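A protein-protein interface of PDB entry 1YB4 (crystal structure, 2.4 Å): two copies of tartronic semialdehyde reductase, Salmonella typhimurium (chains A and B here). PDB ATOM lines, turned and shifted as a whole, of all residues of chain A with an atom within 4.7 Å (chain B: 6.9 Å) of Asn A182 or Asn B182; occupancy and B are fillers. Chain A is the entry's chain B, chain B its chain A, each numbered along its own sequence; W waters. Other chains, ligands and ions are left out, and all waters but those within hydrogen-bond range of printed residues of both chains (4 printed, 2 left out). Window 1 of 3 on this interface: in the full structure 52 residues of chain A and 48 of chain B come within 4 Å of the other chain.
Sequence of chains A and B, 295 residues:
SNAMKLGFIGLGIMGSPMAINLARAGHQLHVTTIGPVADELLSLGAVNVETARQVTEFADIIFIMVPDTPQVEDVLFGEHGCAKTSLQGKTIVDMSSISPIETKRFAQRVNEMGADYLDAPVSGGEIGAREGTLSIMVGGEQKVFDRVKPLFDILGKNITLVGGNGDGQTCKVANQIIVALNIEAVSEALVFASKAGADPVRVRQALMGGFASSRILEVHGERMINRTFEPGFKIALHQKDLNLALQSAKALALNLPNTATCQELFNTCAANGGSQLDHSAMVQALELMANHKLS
Printed residues of chain A that touch a printed residue of chain B: Ile A178, Leu A181, Asn A182, Glu A184, Ala A185, Ala A212, Ser A214 and Ile A216.
Hydrophobic or aromatic side chains of chain B within 4 Å of the printed part of chain A: Ile B178, Leu B181, Ala B185 and Ala B212.
Among the printed residues, no Asp or Glu carboxylate lies within 4 Å of a Lys or Arg side-chain nitrogen of the other chain.
Among the printed residues, pairs that only touch across the chains: Ser A214 with Ser B213 (3.4 Å), Ala A185 with Leu B181 (3.4 Å), Leu A181 with Ala B185 (3.4 Å), Ile A216 with Phe B211 (3.5 Å), Ser A214 with Ser B214 (3.5 Å), Asn A182 with Asn B182 (3.5 Å), Ala A212 with Ile B178 (3.6 Å), Glu A184 with Leu B181 (3.6 Å), Ile A178 with Ala B212 (3.7 Å), Leu A181 with Glu B184 (3.7 Å), Ala A212 with Asn B182 (3.9 Å), Asn A182 with Ala B185 (3.9 Å) and Ala A185 with Ile B178 (3.9 Å).
Asn A182 touches just these residues of chain B: Asn B182 and Ala B185.
Asn B182 touches just these residues of chain A: Asn A182 and Ala A212.
Printed residues of chain B within 4 Å of Ala A185: Ile B178 (3.9 Å) and Leu B181 (3.4 Å).
Of the printed residues of chain B, Ser A214 touches Ser B213 (3.4 Å) and Ser B214 (3.5 Å).
Of the printed residues of chain B, Ile A216 touches Phe B211 (3.5 Å).
Printed residues of chain A within 4 Å of Ala B185: Leu A181 and Asn A182.
Of the printed residues of chain A, Ser B213 touches Ser A214 (3.4 Å).
The nearest residue of chain A that does not touch Asn B182 is Ala A185 (4.1 Å).
The nearest printed residue of chain B that does not touch Ile A178 is Ala B185 (4.02 Å).
Water W3 lies within hydrogen-bond range of the backbone carbonyl oxygen (O) of Ala B212 (2.5 Å), the side-chain amide nitrogen (ND2) of Asn A182 (3.2 Å) and the side-chain hydroxyl (OG) of Ser B214 (3.2 Å).
Water W2 lies within hydrogen-bond range of OG of Ser A214, O of Ala A212 and ND2 of Asn B182.
Water W4 lies within hydrogen-bond range of the backbone carbonyl oxygen of Asn A182 (2.7 Å) and the side-chain amide oxygen of Asn B182 (2.8 Å).
Water W1 lies within hydrogen-bond range of O of Phe B211, O of Ser B213, N of Ile A216, ND2 of Asn A182 and OG of Ser A214.
Leu A181 touches Glu B184, and with the chains exchanged Glu A184 touches Leu B181.
Asn A182 touches Ala B185, but with the chains exchanged Ala A185 does not touch Asn B182 (4.1 Å).
Ala A185 touches Ile B178, but with the chains exchanged Ile A178 does not touch Ala B185 (4.02 Å).
Ser B214 touches its own counterpart, Ser A214.
Of the 13 pairs that touch across the chains among the printed residues, 8 have their exchanged pair printed and touching as well.
OD1 of Asn B182 lies close to O of Ile B178 (3.3 Å).
The side-chain hydroxyl (OG) of Ser B214 is in hydrogen-bond range of the backbone NH (N) of Ile B216 (2.9 Å).
OG of Ser B214 is in hydrogen-bond range of N of Leu B217, at 2.6 Å.
O of Ile A178 sits close to OD1 of Asn A182, at 3.1 Å.
The backbone NH (N) of Ile A216 lies close to the side-chain hydroxyl (OG) of Ser A214 (3.4 Å).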
ATOM      1  N   ILE A 178      18.863  -5.521 -16.717  1.00  0.00           N
ATOM      2  CA  ILE A 178      18.234  -5.316 -15.417  1.00  0.00           C
ATOM      3  C   ILE A 178      18.939  -6.102 -14.323  1.00  0.00           C
ATOM      4  O   ILE A 178      19.208  -5.568 -13.247  1.00  0.00           O
ATOM      5  CB  ILE A 178      16.730  -5.705 -15.438  1.00  0.00           C
ATOM      6  CG1 ILE A 178      15.929  -4.629 -16.181  1.00  0.00           C
ATOM      7  CG2 ILE A 178      16.215  -5.873 -14.012  1.00  0.00           C
ATOM      8  CD1 ILE A 178      14.424  -4.851 -16.221  1.00  0.00           C
ATOM      9  N   VAL A 179      19.249  -7.363 -14.602  1.00  0.00           N
ATOM     10  CA  VAL A 179      19.929  -8.204 -13.622  1.00  0.00           C
ATOM     11  C   VAL A 179      21.248  -7.587 -13.204  1.00  0.00           C
ATOM     12  O   VAL A 179      21.584  -7.560 -12.025  1.00  0.00           O
ATOM     13  CB  VAL A 179      20.193  -9.604 -14.193  1.00  0.00           C
ATOM     14  CG1 VAL A 179      21.169 -10.367 -13.307  1.00  0.00           C
ATOM     15  CG2 VAL A 179      18.883 -10.341 -14.327  1.00  0.00           C
ATOM     16  N   ALA A 180      21.990  -7.098 -14.195  1.00  0.00           N
ATOM     17  CA  ALA A 180      23.280  -6.473 -13.966  1.00  0.00           C
ATOM     18  C   ALA A 180      23.131  -5.143 -13.207  1.00  0.00           C
ATOM     19  O   ALA A 180      23.865  -4.873 -12.249  1.00  0.00           O
ATOM     20  CB  ALA A 180      23.973  -6.248 -15.299  1.00  0.00           C
ATOM     21  N   LEU A 181      22.188  -4.309 -13.635  1.00  0.00           N
ATOM     22  CA  LEU A 181      21.976  -3.037 -12.972  1.00  0.00           C
ATOM     23  C   LEU A 181      21.446  -3.265 -11.548  1.00  0.00           C
ATOM     24  O   LEU A 181      21.865  -2.577 -10.617  1.00  0.00           O
ATOM     25  CB  LEU A 181      21.023  -2.168 -13.811  1.00  0.00           C
ATOM     26  CG  LEU A 181      21.706  -1.208 -14.806  1.00  0.00           C
ATOM     27  CD1 LEU A 181      22.639  -1.965 -15.728  1.00  0.00           C
ATOM     28  CD2 LEU A 181      20.662  -0.450 -15.605  1.00  0.00           C
ATOM     29  N   ASN A 182      20.540  -4.234 -11.371  1.00  0.00           N
ATOM     30  CA  ASN A 182      19.995  -4.537 -10.046  1.00  0.00           C
ATOM     31  C   ASN A 182      21.066  -5.021  -9.076  1.00  0.00           C
ATOM     32  O   ASN A 182      21.058  -4.645  -7.910  1.00  0.00           O
ATOM     33  CB  ASN A 182      18.892  -5.582 -10.142  1.00  0.00           C
ATOM     34  CG  ASN A 182      17.599  -5.001 -10.641  1.00  0.00           C
ATOM     35  OD1 ASN A 182      17.579  -3.891 -11.142  1.00  0.00           O
ATOM     36  ND2 ASN A 182      16.513  -5.751 -10.514  1.00  0.00           N
ATOM     37  N   ILE A 183      21.974  -5.864  -9.555  1.00  0.00           N
ATOM     38  CA  ILE A 183      23.065  -6.359  -8.731  1.00  0.00           C
ATOM     39  C   ILE A 183      23.969  -5.207  -8.299  1.00  0.00           C
ATOM     40  O   ILE A 183      24.423  -5.164  -7.154  1.00  0.00           O
ATOM     41  CB  ILE A 183      23.932  -7.377  -9.490  1.00  0.00           C
ATOM     42  CG1 ILE A 183      23.132  -8.667  -9.709  1.00  0.00           C
ATOM     43  CG2 ILE A 183      25.218  -7.640  -8.706  1.00  0.00           C
ATOM     44  CD1 ILE A 183      23.830  -9.729 -10.552  1.00  0.00           C
ATOM     45  N   GLU A 184      24.221  -4.271  -9.213  1.00  0.00           N
ATOM     46  CA  GLU A 184      25.092  -3.130  -8.934  1.00  0.00           C
ATOM     47  C   GLU A 184      24.458  -2.182  -7.919  1.00  0.00           C
ATOM     48  O   GLU A 184      25.145  -1.618  -7.063  1.00  0.00           O
ATOM     49  CB  GLU A 184      25.392  -2.384 -10.244  1.00  0.00           C
ATOM     50  CG  GLU A 184      26.568  -1.404 -10.206  1.00  0.00           C
ATOM     51  CD  GLU A 184      26.288  -0.143  -9.409  1.00  0.00           C
ATOM     52  OE1 GLU A 184      25.105   0.175  -9.176  1.00  0.00           O
ATOM     53  OE2 GLU A 184      27.256   0.540  -9.031  1.00  0.00           O
ATOM     54  N   ALA A 185      23.145  -2.004  -8.016  1.00  0.00           N
ATOM     55  CA  ALA A 185      22.441  -1.130  -7.089  1.00  0.00           C
ATOM     56  C   ALA A 185      22.477  -1.707  -5.677  1.00  0.00           C
ATOM     57  O   ALA A 185      22.738  -0.994  -4.712  1.00  0.00           O
ATOM     58  CB  ALA A 185      21.002  -0.939  -7.533  1.00  0.00           C
ATOM     59  N   VAL A 186      22.204  -2.996  -5.540  1.00  0.00           N
ATOM     60  CA  VAL A 186      22.239  -3.569  -4.209  1.00  0.00           C
ATOM     61  C   VAL A 186      23.647  -3.360  -3.656  1.00  0.00           C
ATOM     62  O   VAL A 186      23.805  -3.027  -2.491  1.00  0.00           O
ATOM     63  CB  VAL A 186      21.880  -5.075  -4.212  1.00  0.00           C
ATOM     64  CG1 VAL A 186      21.914  -5.622  -2.788  1.00  0.00           C
ATOM     65  CG2 VAL A 186      20.489  -5.266  -4.816  1.00  0.00           C
ATOM     66  N   ALA A 212      12.120  -1.246  -2.751  1.00  0.00           N
ATOM     67  CA  ALA A 212      13.488  -1.648  -3.042  1.00  0.00           C
ATOM     68  C   ALA A 212      13.504  -3.145  -3.380  1.00  0.00           C
ATOM     69  O   ALA A 212      14.438  -3.644  -4.010  1.00  0.00           O
ATOM     70  CB  ALA A 212      14.379  -1.372  -1.839  1.00  0.00           C
ATOM     71  N   SER A 214      13.250  -6.819  -4.790  1.00  0.00           N
ATOM     72  CA  SER A 214      13.480  -7.452  -6.084  1.00  0.00           C
ATOM     73  C   SER A 214      14.114  -8.809  -5.794  1.00  0.00           C
ATOM     74  O   SER A 214      14.589  -9.053  -4.681  1.00  0.00           O
ATOM     75  CB  SER A 214      14.450  -6.631  -6.922  1.00  0.00           C
ATOM     76  OG  SER A 214      15.759  -6.713  -6.370  1.00  0.00           O
ATOM     77  N   ILE A 216      16.867  -9.913  -6.917  1.00  0.00           N
ATOM     78  CA  ILE A 216      18.306  -9.715  -6.749  1.00  0.00           C
ATOM     79  C   ILE A 216      18.622  -9.373  -5.298  1.00  0.00           C
ATOM     80  O   ILE A 216      19.542  -9.926  -4.699  1.00  0.00           O
ATOM     81  CB  ILE A 216      18.836  -8.566  -7.668  1.00  0.00           C
ATOM     82  CG1 ILE A 216      18.769  -8.995  -9.134  1.00  0.00           C
ATOM     83  CG2 ILE A 216      20.271  -8.213  -7.309  1.00  0.00           C
ATOM     84  CD1 ILE A 216      19.676 -10.156  -9.481  1.00  0.00           C
ATOM     85  N   ILE B 177      18.350   4.897  -2.826  1.00  0.00           N
ATOM     86  CA  ILE B 177      19.343   4.612  -3.862  1.00  0.00           C
ATOM     87  C   ILE B 177      18.829   3.493  -4.773  1.00  0.00           C
ATOM     88  O   ILE B 177      18.843   3.617  -5.993  1.00  0.00           O
ATOM     89  CB  ILE B 177      20.695   4.149  -3.268  1.00  0.00           C
ATOM     90  CG1 ILE B 177      21.447   5.324  -2.656  1.00  0.00           C
ATOM     91  CG2 ILE B 177      21.537   3.514  -4.343  1.00  0.00           C
ATOM     92  CD1 ILE B 177      22.702   4.907  -1.919  1.00  0.00           C
ATOM     93  N   ILE B 178      18.373   2.401  -4.170  1.00  0.00           N
ATOM     94  CA  ILE B 178      17.883   1.262  -4.924  1.00  0.00           C
ATOM     95  C   ILE B 178      16.629   1.592  -5.706  1.00  0.00           C
ATOM     96  O   ILE B 178      16.475   1.136  -6.828  1.00  0.00           O
ATOM     97  CB  ILE B 178      17.628   0.060  -3.998  1.00  0.00           C
ATOM     98  CG1 ILE B 178      18.980  -0.558  -3.605  1.00  0.00           C
ATOM     99  CG2 ILE B 178      16.689  -0.951  -4.662  1.00  0.00           C
ATOM    100  CD1 ILE B 178      18.904  -1.812  -2.763  1.00  0.00           C
ATOM    101  N   VAL B 179      15.730   2.388  -5.141  1.00  0.00           N
ATOM    102  CA  VAL B 179      14.523   2.716  -5.882  1.00  0.00           C
ATOM    103  C   VAL B 179      14.909   3.478  -7.131  1.00  0.00           C
ATOM    104  O   VAL B 179      14.358   3.240  -8.208  1.00  0.00           O
ATOM    105  CB  VAL B 179      13.544   3.556  -5.039  1.00  0.00           C
ATOM    106  CG1 VAL B 179      12.278   3.883  -5.851  1.00  0.00           C
ATOM    107  CG2 VAL B 179      13.179   2.783  -3.788  1.00  0.00           C
ATOM    108  N   ALA B 180      15.877   4.378  -6.991  1.00  0.00           N
ATOM    109  CA  ALA B 180      16.346   5.182  -8.118  1.00  0.00           C
ATOM    110  C   ALA B 180      17.062   4.308  -9.153  1.00  0.00           C
ATOM    111  O   ALA B 180      16.729   4.318 -10.340  1.00  0.00           O
ATOM    112  CB  ALA B 180      17.281   6.285  -7.622  1.00  0.00           C
ATOM    113  N   LEU B 181      18.055   3.553  -8.707  1.00  0.00           N
ATOM    114  CA  LEU B 181      18.770   2.697  -9.623  1.00  0.00           C
ATOM    115  C   LEU B 181      17.860   1.647 -10.299  1.00  0.00           C
ATOM    116  O   LEU B 181      18.039   1.356 -11.483  1.00  0.00           O
ATOM    117  CB  LEU B 181      19.959   2.042  -8.899  1.00  0.00           C
ATOM    118  CG  LEU B 181      21.199   2.945  -8.927  1.00  0.00           C
ATOM    119  CD1 LEU B 181      20.863   4.312  -8.325  1.00  0.00           C
ATOM    120  CD2 LEU B 181      22.335   2.278  -8.176  1.00  0.00           C
ATOM    121  N   ASN B 182      16.885   1.092  -9.568  1.00  0.00           N
ATOM    122  CA  ASN B 182      15.972   0.091 -10.149  1.00  0.00           C
ATOM    123  C   ASN B 182      15.072   0.751 -11.191  1.00  0.00           C
ATOM    124  O   ASN B 182      14.844   0.188 -12.271  1.00  0.00           O
ATOM    125  CB  ASN B 182      15.126  -0.567  -9.065  1.00  0.00           C
ATOM    126  CG  ASN B 182      15.860  -1.686  -8.370  1.00  0.00           C
ATOM    127  OD1 ASN B 182      17.092  -1.739  -8.397  1.00  0.00           O
ATOM    128  ND2 ASN B 182      15.114  -2.587  -7.734  1.00  0.00           N
ATOM    129  N   ILE B 183      14.584   1.952 -10.885  1.00  0.00           N
ATOM    130  CA  ILE B 183      13.737   2.670 -11.833  1.00  0.00           C
ATOM    131  C   ILE B 183      14.529   2.959 -13.107  1.00  0.00           C
ATOM    132  O   ILE B 183      14.017   2.803 -14.214  1.00  0.00           O
ATOM    133  CB  ILE B 183      13.207   4.016 -11.244  1.00  0.00           C
ATOM    134  CG1 ILE B 183      12.188   3.730 -10.137  1.00  0.00           C
ATOM    135  CG2 ILE B 183      12.540   4.834 -12.327  1.00  0.00           C
ATOM    136  CD1 ILE B 183      11.734   4.975  -9.349  1.00  0.00           C
ATOM    137  N   GLU B 184      15.787   3.360 -12.959  1.00  0.00           N
ATOM    138  CA  GLU B 184      16.599   3.674 -14.121  1.00  0.00           C
ATOM    139  C   GLU B 184      16.878   2.402 -14.917  1.00  0.00           C
ATOM    140  O   GLU B 184      16.907   2.419 -16.153  1.00  0.00           O
ATOM    141  CB  GLU B 184      17.900   4.341 -13.677  1.00  0.00           C
ATOM    142  CG  GLU B 184      18.605   5.163 -14.754  1.00  0.00           C
ATOM    143  CD  GLU B 184      19.483   4.328 -15.665  1.00  0.00           C
ATOM    144  OE1 GLU B 184      19.834   3.188 -15.282  1.00  0.00           O
ATOM    145  OE2 GLU B 184      19.842   4.826 -16.757  1.00  0.00           O
ATOM    146  N   ALA B 185      17.064   1.295 -14.212  1.00  0.00           N
ATOM    147  CA  ALA B 185      17.328   0.033 -14.886  1.00  0.00           C
ATOM    148  C   ALA B 185      16.151  -0.381 -15.778  1.00  0.00           C
ATOM    149  O   ALA B 185      16.335  -0.705 -16.951  1.00  0.00           O
ATOM    150  CB  ALA B 185      17.645  -1.053 -13.868  1.00  0.00           C
ATOM    151  N   VAL B 186      14.942  -0.367 -15.228  1.00  0.00           N
ATOM    152  CA  VAL B 186      13.761  -0.732 -16.010  1.00  0.00           C
ATOM    153  C   VAL B 186      13.646   0.201 -17.230  1.00  0.00           C
ATOM    154  O   VAL B 186      13.250  -0.232 -18.320  1.00  0.00           O
ATOM    155  CB  VAL B 186      12.468  -0.647 -15.134  1.00  0.00           C
ATOM    156  CG1 VAL B 186      11.246  -1.139 -15.916  1.00  0.00           C
ATOM    157  CG2 VAL B 186      12.663  -1.492 -13.870  1.00  0.00           C
ATOM    158  N   SER B 187      14.017   1.469 -17.051  1.00  0.00           N
ATOM    159  CA  SER B 187      13.968   2.465 -18.131  1.00  0.00           C
ATOM    160  C   SER B 187      14.923   2.136 -19.295  1.00  0.00           C
ATOM    161  O   SER B 187      14.563   2.256 -20.471  1.00  0.00           O
ATOM    162  CB  SER B 187      14.330   3.851 -17.580  1.00  0.00           C
ATOM    163  OG  SER B 187      13.500   4.225 -16.491  1.00  0.00           O
ATOM    164  N   PHE B 211      15.048 -13.482 -12.640  1.00  0.00           N
ATOM    165  CA  PHE B 211      15.859 -12.649 -11.759  1.00  0.00           C
ATOM    166  C   PHE B 211      15.752 -11.147 -11.945  1.00  0.00           C
ATOM    167  O   PHE B 211      16.257 -10.382 -11.121  1.00  0.00           O
ATOM    168  CB  PHE B 211      17.312 -13.093 -11.821  1.00  0.00           C
ATOM    169  CG  PHE B 211      17.610 -14.228 -10.894  1.00  0.00           C
ATOM    170  CD1 PHE B 211      18.210 -13.998  -9.668  1.00  0.00           C
ATOM    171  CD2 PHE B 211      17.193 -15.517 -11.202  1.00  0.00           C
ATOM    172  CE1 PHE B 211      18.386 -15.038  -8.753  1.00  0.00           C
ATOM    173  CE2 PHE B 211      17.364 -16.557 -10.296  1.00  0.00           C
ATOM    174  CZ  PHE B 211      17.960 -16.313  -9.069  1.00  0.00           C
ATOM    175  N   ALA B 212      15.073 -10.734 -13.010  1.00  0.00           N
ATOM    176  CA  ALA B 212      14.865  -9.320 -13.293  1.00  0.00           C
ATOM    177  C   ALA B 212      13.672  -8.830 -12.477  1.00  0.00           C
ATOM    178  O   ALA B 212      13.450  -7.628 -12.331  1.00  0.00           O
ATOM    179  CB  ALA B 212      14.596  -9.121 -14.778  1.00  0.00           C
ATOM    180  N   SER B 213      12.906  -9.778 -11.946  1.00  0.00           N
ATOM    181  CA  SER B 213      11.723  -9.466 -11.140  1.00  0.00           C
ATOM    182  C   SER B 213      12.000  -8.470 -10.017  1.00  0.00           C
ATOM    183  O   SER B 213      12.927  -8.649  -9.225  1.00  0.00           O
ATOM    184  CB  SER B 213      11.143 -10.749 -10.536  1.00  0.00           C
ATOM    185  OG  SER B 213      10.040 -10.475  -9.694  1.00  0.00           O
ATOM    186  N   SER B 214      11.181  -7.424  -9.956  1.00  0.00           N
ATOM    187  CA  SER B 214      11.320  -6.411  -8.924  1.00  0.00           C
ATOM    188  C   SER B 214       9.980  -5.759  -8.613  1.00  0.00           C
ATOM    189  O   SER B 214       9.032  -5.839  -9.402  1.00  0.00           O
ATOM    190  CB  SER B 214      12.299  -5.314  -9.367  1.00  0.00           C
ATOM    191  OG  SER B 214      11.633  -4.284 -10.090  1.00  0.00           O
ATOM    192  N   ARG B 215       9.919  -5.091  -7.465  1.00  0.00           N
ATOM    193  CA  ARG B 215       8.717  -4.389  -7.048  1.00  0.00           C
ATOM    194  C   ARG B 215       8.575  -3.142  -7.918  1.00  0.00           C
ATOM    195  O   ARG B 215       7.477  -2.591  -8.058  1.00  0.00           O
ATOM    196  CB  ARG B 215       8.840  -4.006  -5.577  1.00  0.00           C
ATOM    197  CG  ARG B 215       7.650  -3.286  -5.010  1.00  0.00           C
ATOM    198  CD  ARG B 215       6.362  -4.062  -5.196  1.00  0.00           C
ATOM    199  NE  ARG B 215       5.263  -3.374  -4.527  1.00  0.00           N
ATOM    200  CZ  ARG B 215       3.978  -3.532  -4.827  1.00  0.00           C
ATOM    201  NH1 ARG B 215       3.609  -4.365  -5.801  1.00  0.00           N
ATOM    202  NH2 ARG B 215       3.058  -2.856  -4.148  1.00  0.00           N
ATOM    203  N   ILE B 216       9.701  -2.726  -8.509  1.00  0.00           N
ATOM    204  CA  ILE B 216       9.784  -1.557  -9.389  1.00  0.00           C
ATOM    205  C   ILE B 216       9.326  -1.863 -10.817  1.00  0.00           C
ATOM    206  O   ILE B 216       8.592  -1.073 -11.413  1.00  0.00           O
ATOM    207  CB  ILE B 216      11.239  -1.010  -9.460  1.00  0.00           C
ATOM    208  CG1 ILE B 216      11.637  -0.430  -8.105  1.00  0.00           C
ATOM    209  CG2 ILE B 216      11.365   0.048 -10.571  1.00  0.00           C
ATOM    210  CD1 ILE B 216      10.781   0.715  -7.683  1.00  0.00           C
ATOM    211  N   LEU B 217       9.790  -2.978 -11.380  1.00  0.00           N
ATOM    212  CA  LEU B 217       9.376  -3.365 -12.726  1.00  0.00           C
ATOM    213  C   LEU B 217       7.870  -3.624 -12.732  1.00  0.00           C
ATOM    214  O   LEU B 217       7.177  -3.338 -13.700  1.00  0.00           O
ATOM    215  CB  LEU B 217      10.102  -4.635 -13.159  1.00  0.00           C
ATOM    216  CG  LEU B 217       9.624  -5.291 -14.457  1.00  0.00           C
ATOM    217  CD1 LEU B 217       9.886  -4.352 -15.636  1.00  0.00           C
ATOM    218  CD2 LEU B 217      10.332  -6.629 -14.649  1.00  0.00           C
ATOM    219  N   MET B 224       5.282   3.344 -16.705  1.00  0.00           N
ATOM    220  CA  MET B 224       6.019   3.826 -17.870  1.00  0.00           C
ATOM    221  C   MET B 224       5.332   3.490 -19.179  1.00  0.00           C
ATOM    222  O   MET B 224       5.353   4.282 -20.128  1.00  0.00           O
ATOM    223  CB  MET B 224       7.436   3.241 -17.881  1.00  0.00           C
ATOM    224  CG  MET B 224       8.352   3.720 -16.747  1.00  0.00           C
ATOM    225  SD  MET B 224      10.079   2.773 -16.692  1.00  0.00           S
ATOM    226  CE  MET B 224      10.361   2.772 -14.763  1.00  0.00           C
ATOM    227  N   CYS B 262      22.273   8.712 -11.818  1.00  0.00           N
ATOM    228  CA  CYS B 262      20.824   8.851 -11.648  1.00  0.00           C
ATOM    229  C   CYS B 262      20.429  10.268 -11.275  1.00  0.00           C
ATOM    230  O   CYS B 262      19.416  10.781 -11.753  1.00  0.00           O
ATOM    231  CB  CYS B 262      20.296   7.879 -10.591  1.00  0.00           C
ATOM    232  SG  CYS B 262      19.976   6.238 -11.269  1.00  0.00           S
HETATM  233  O   HOH W   1      15.724  -8.530  -9.187  1.00  0.00           O
HETATM  234  O   HOH W   2      16.558  -4.330  -5.609  1.00  0.00           O
HETATM  235  O   HOH W   3      13.886  -5.157 -12.231  1.00  0.00           O
HETATM  236  O   HOH W   4      18.822  -3.526  -7.022  1.00  0.00           O
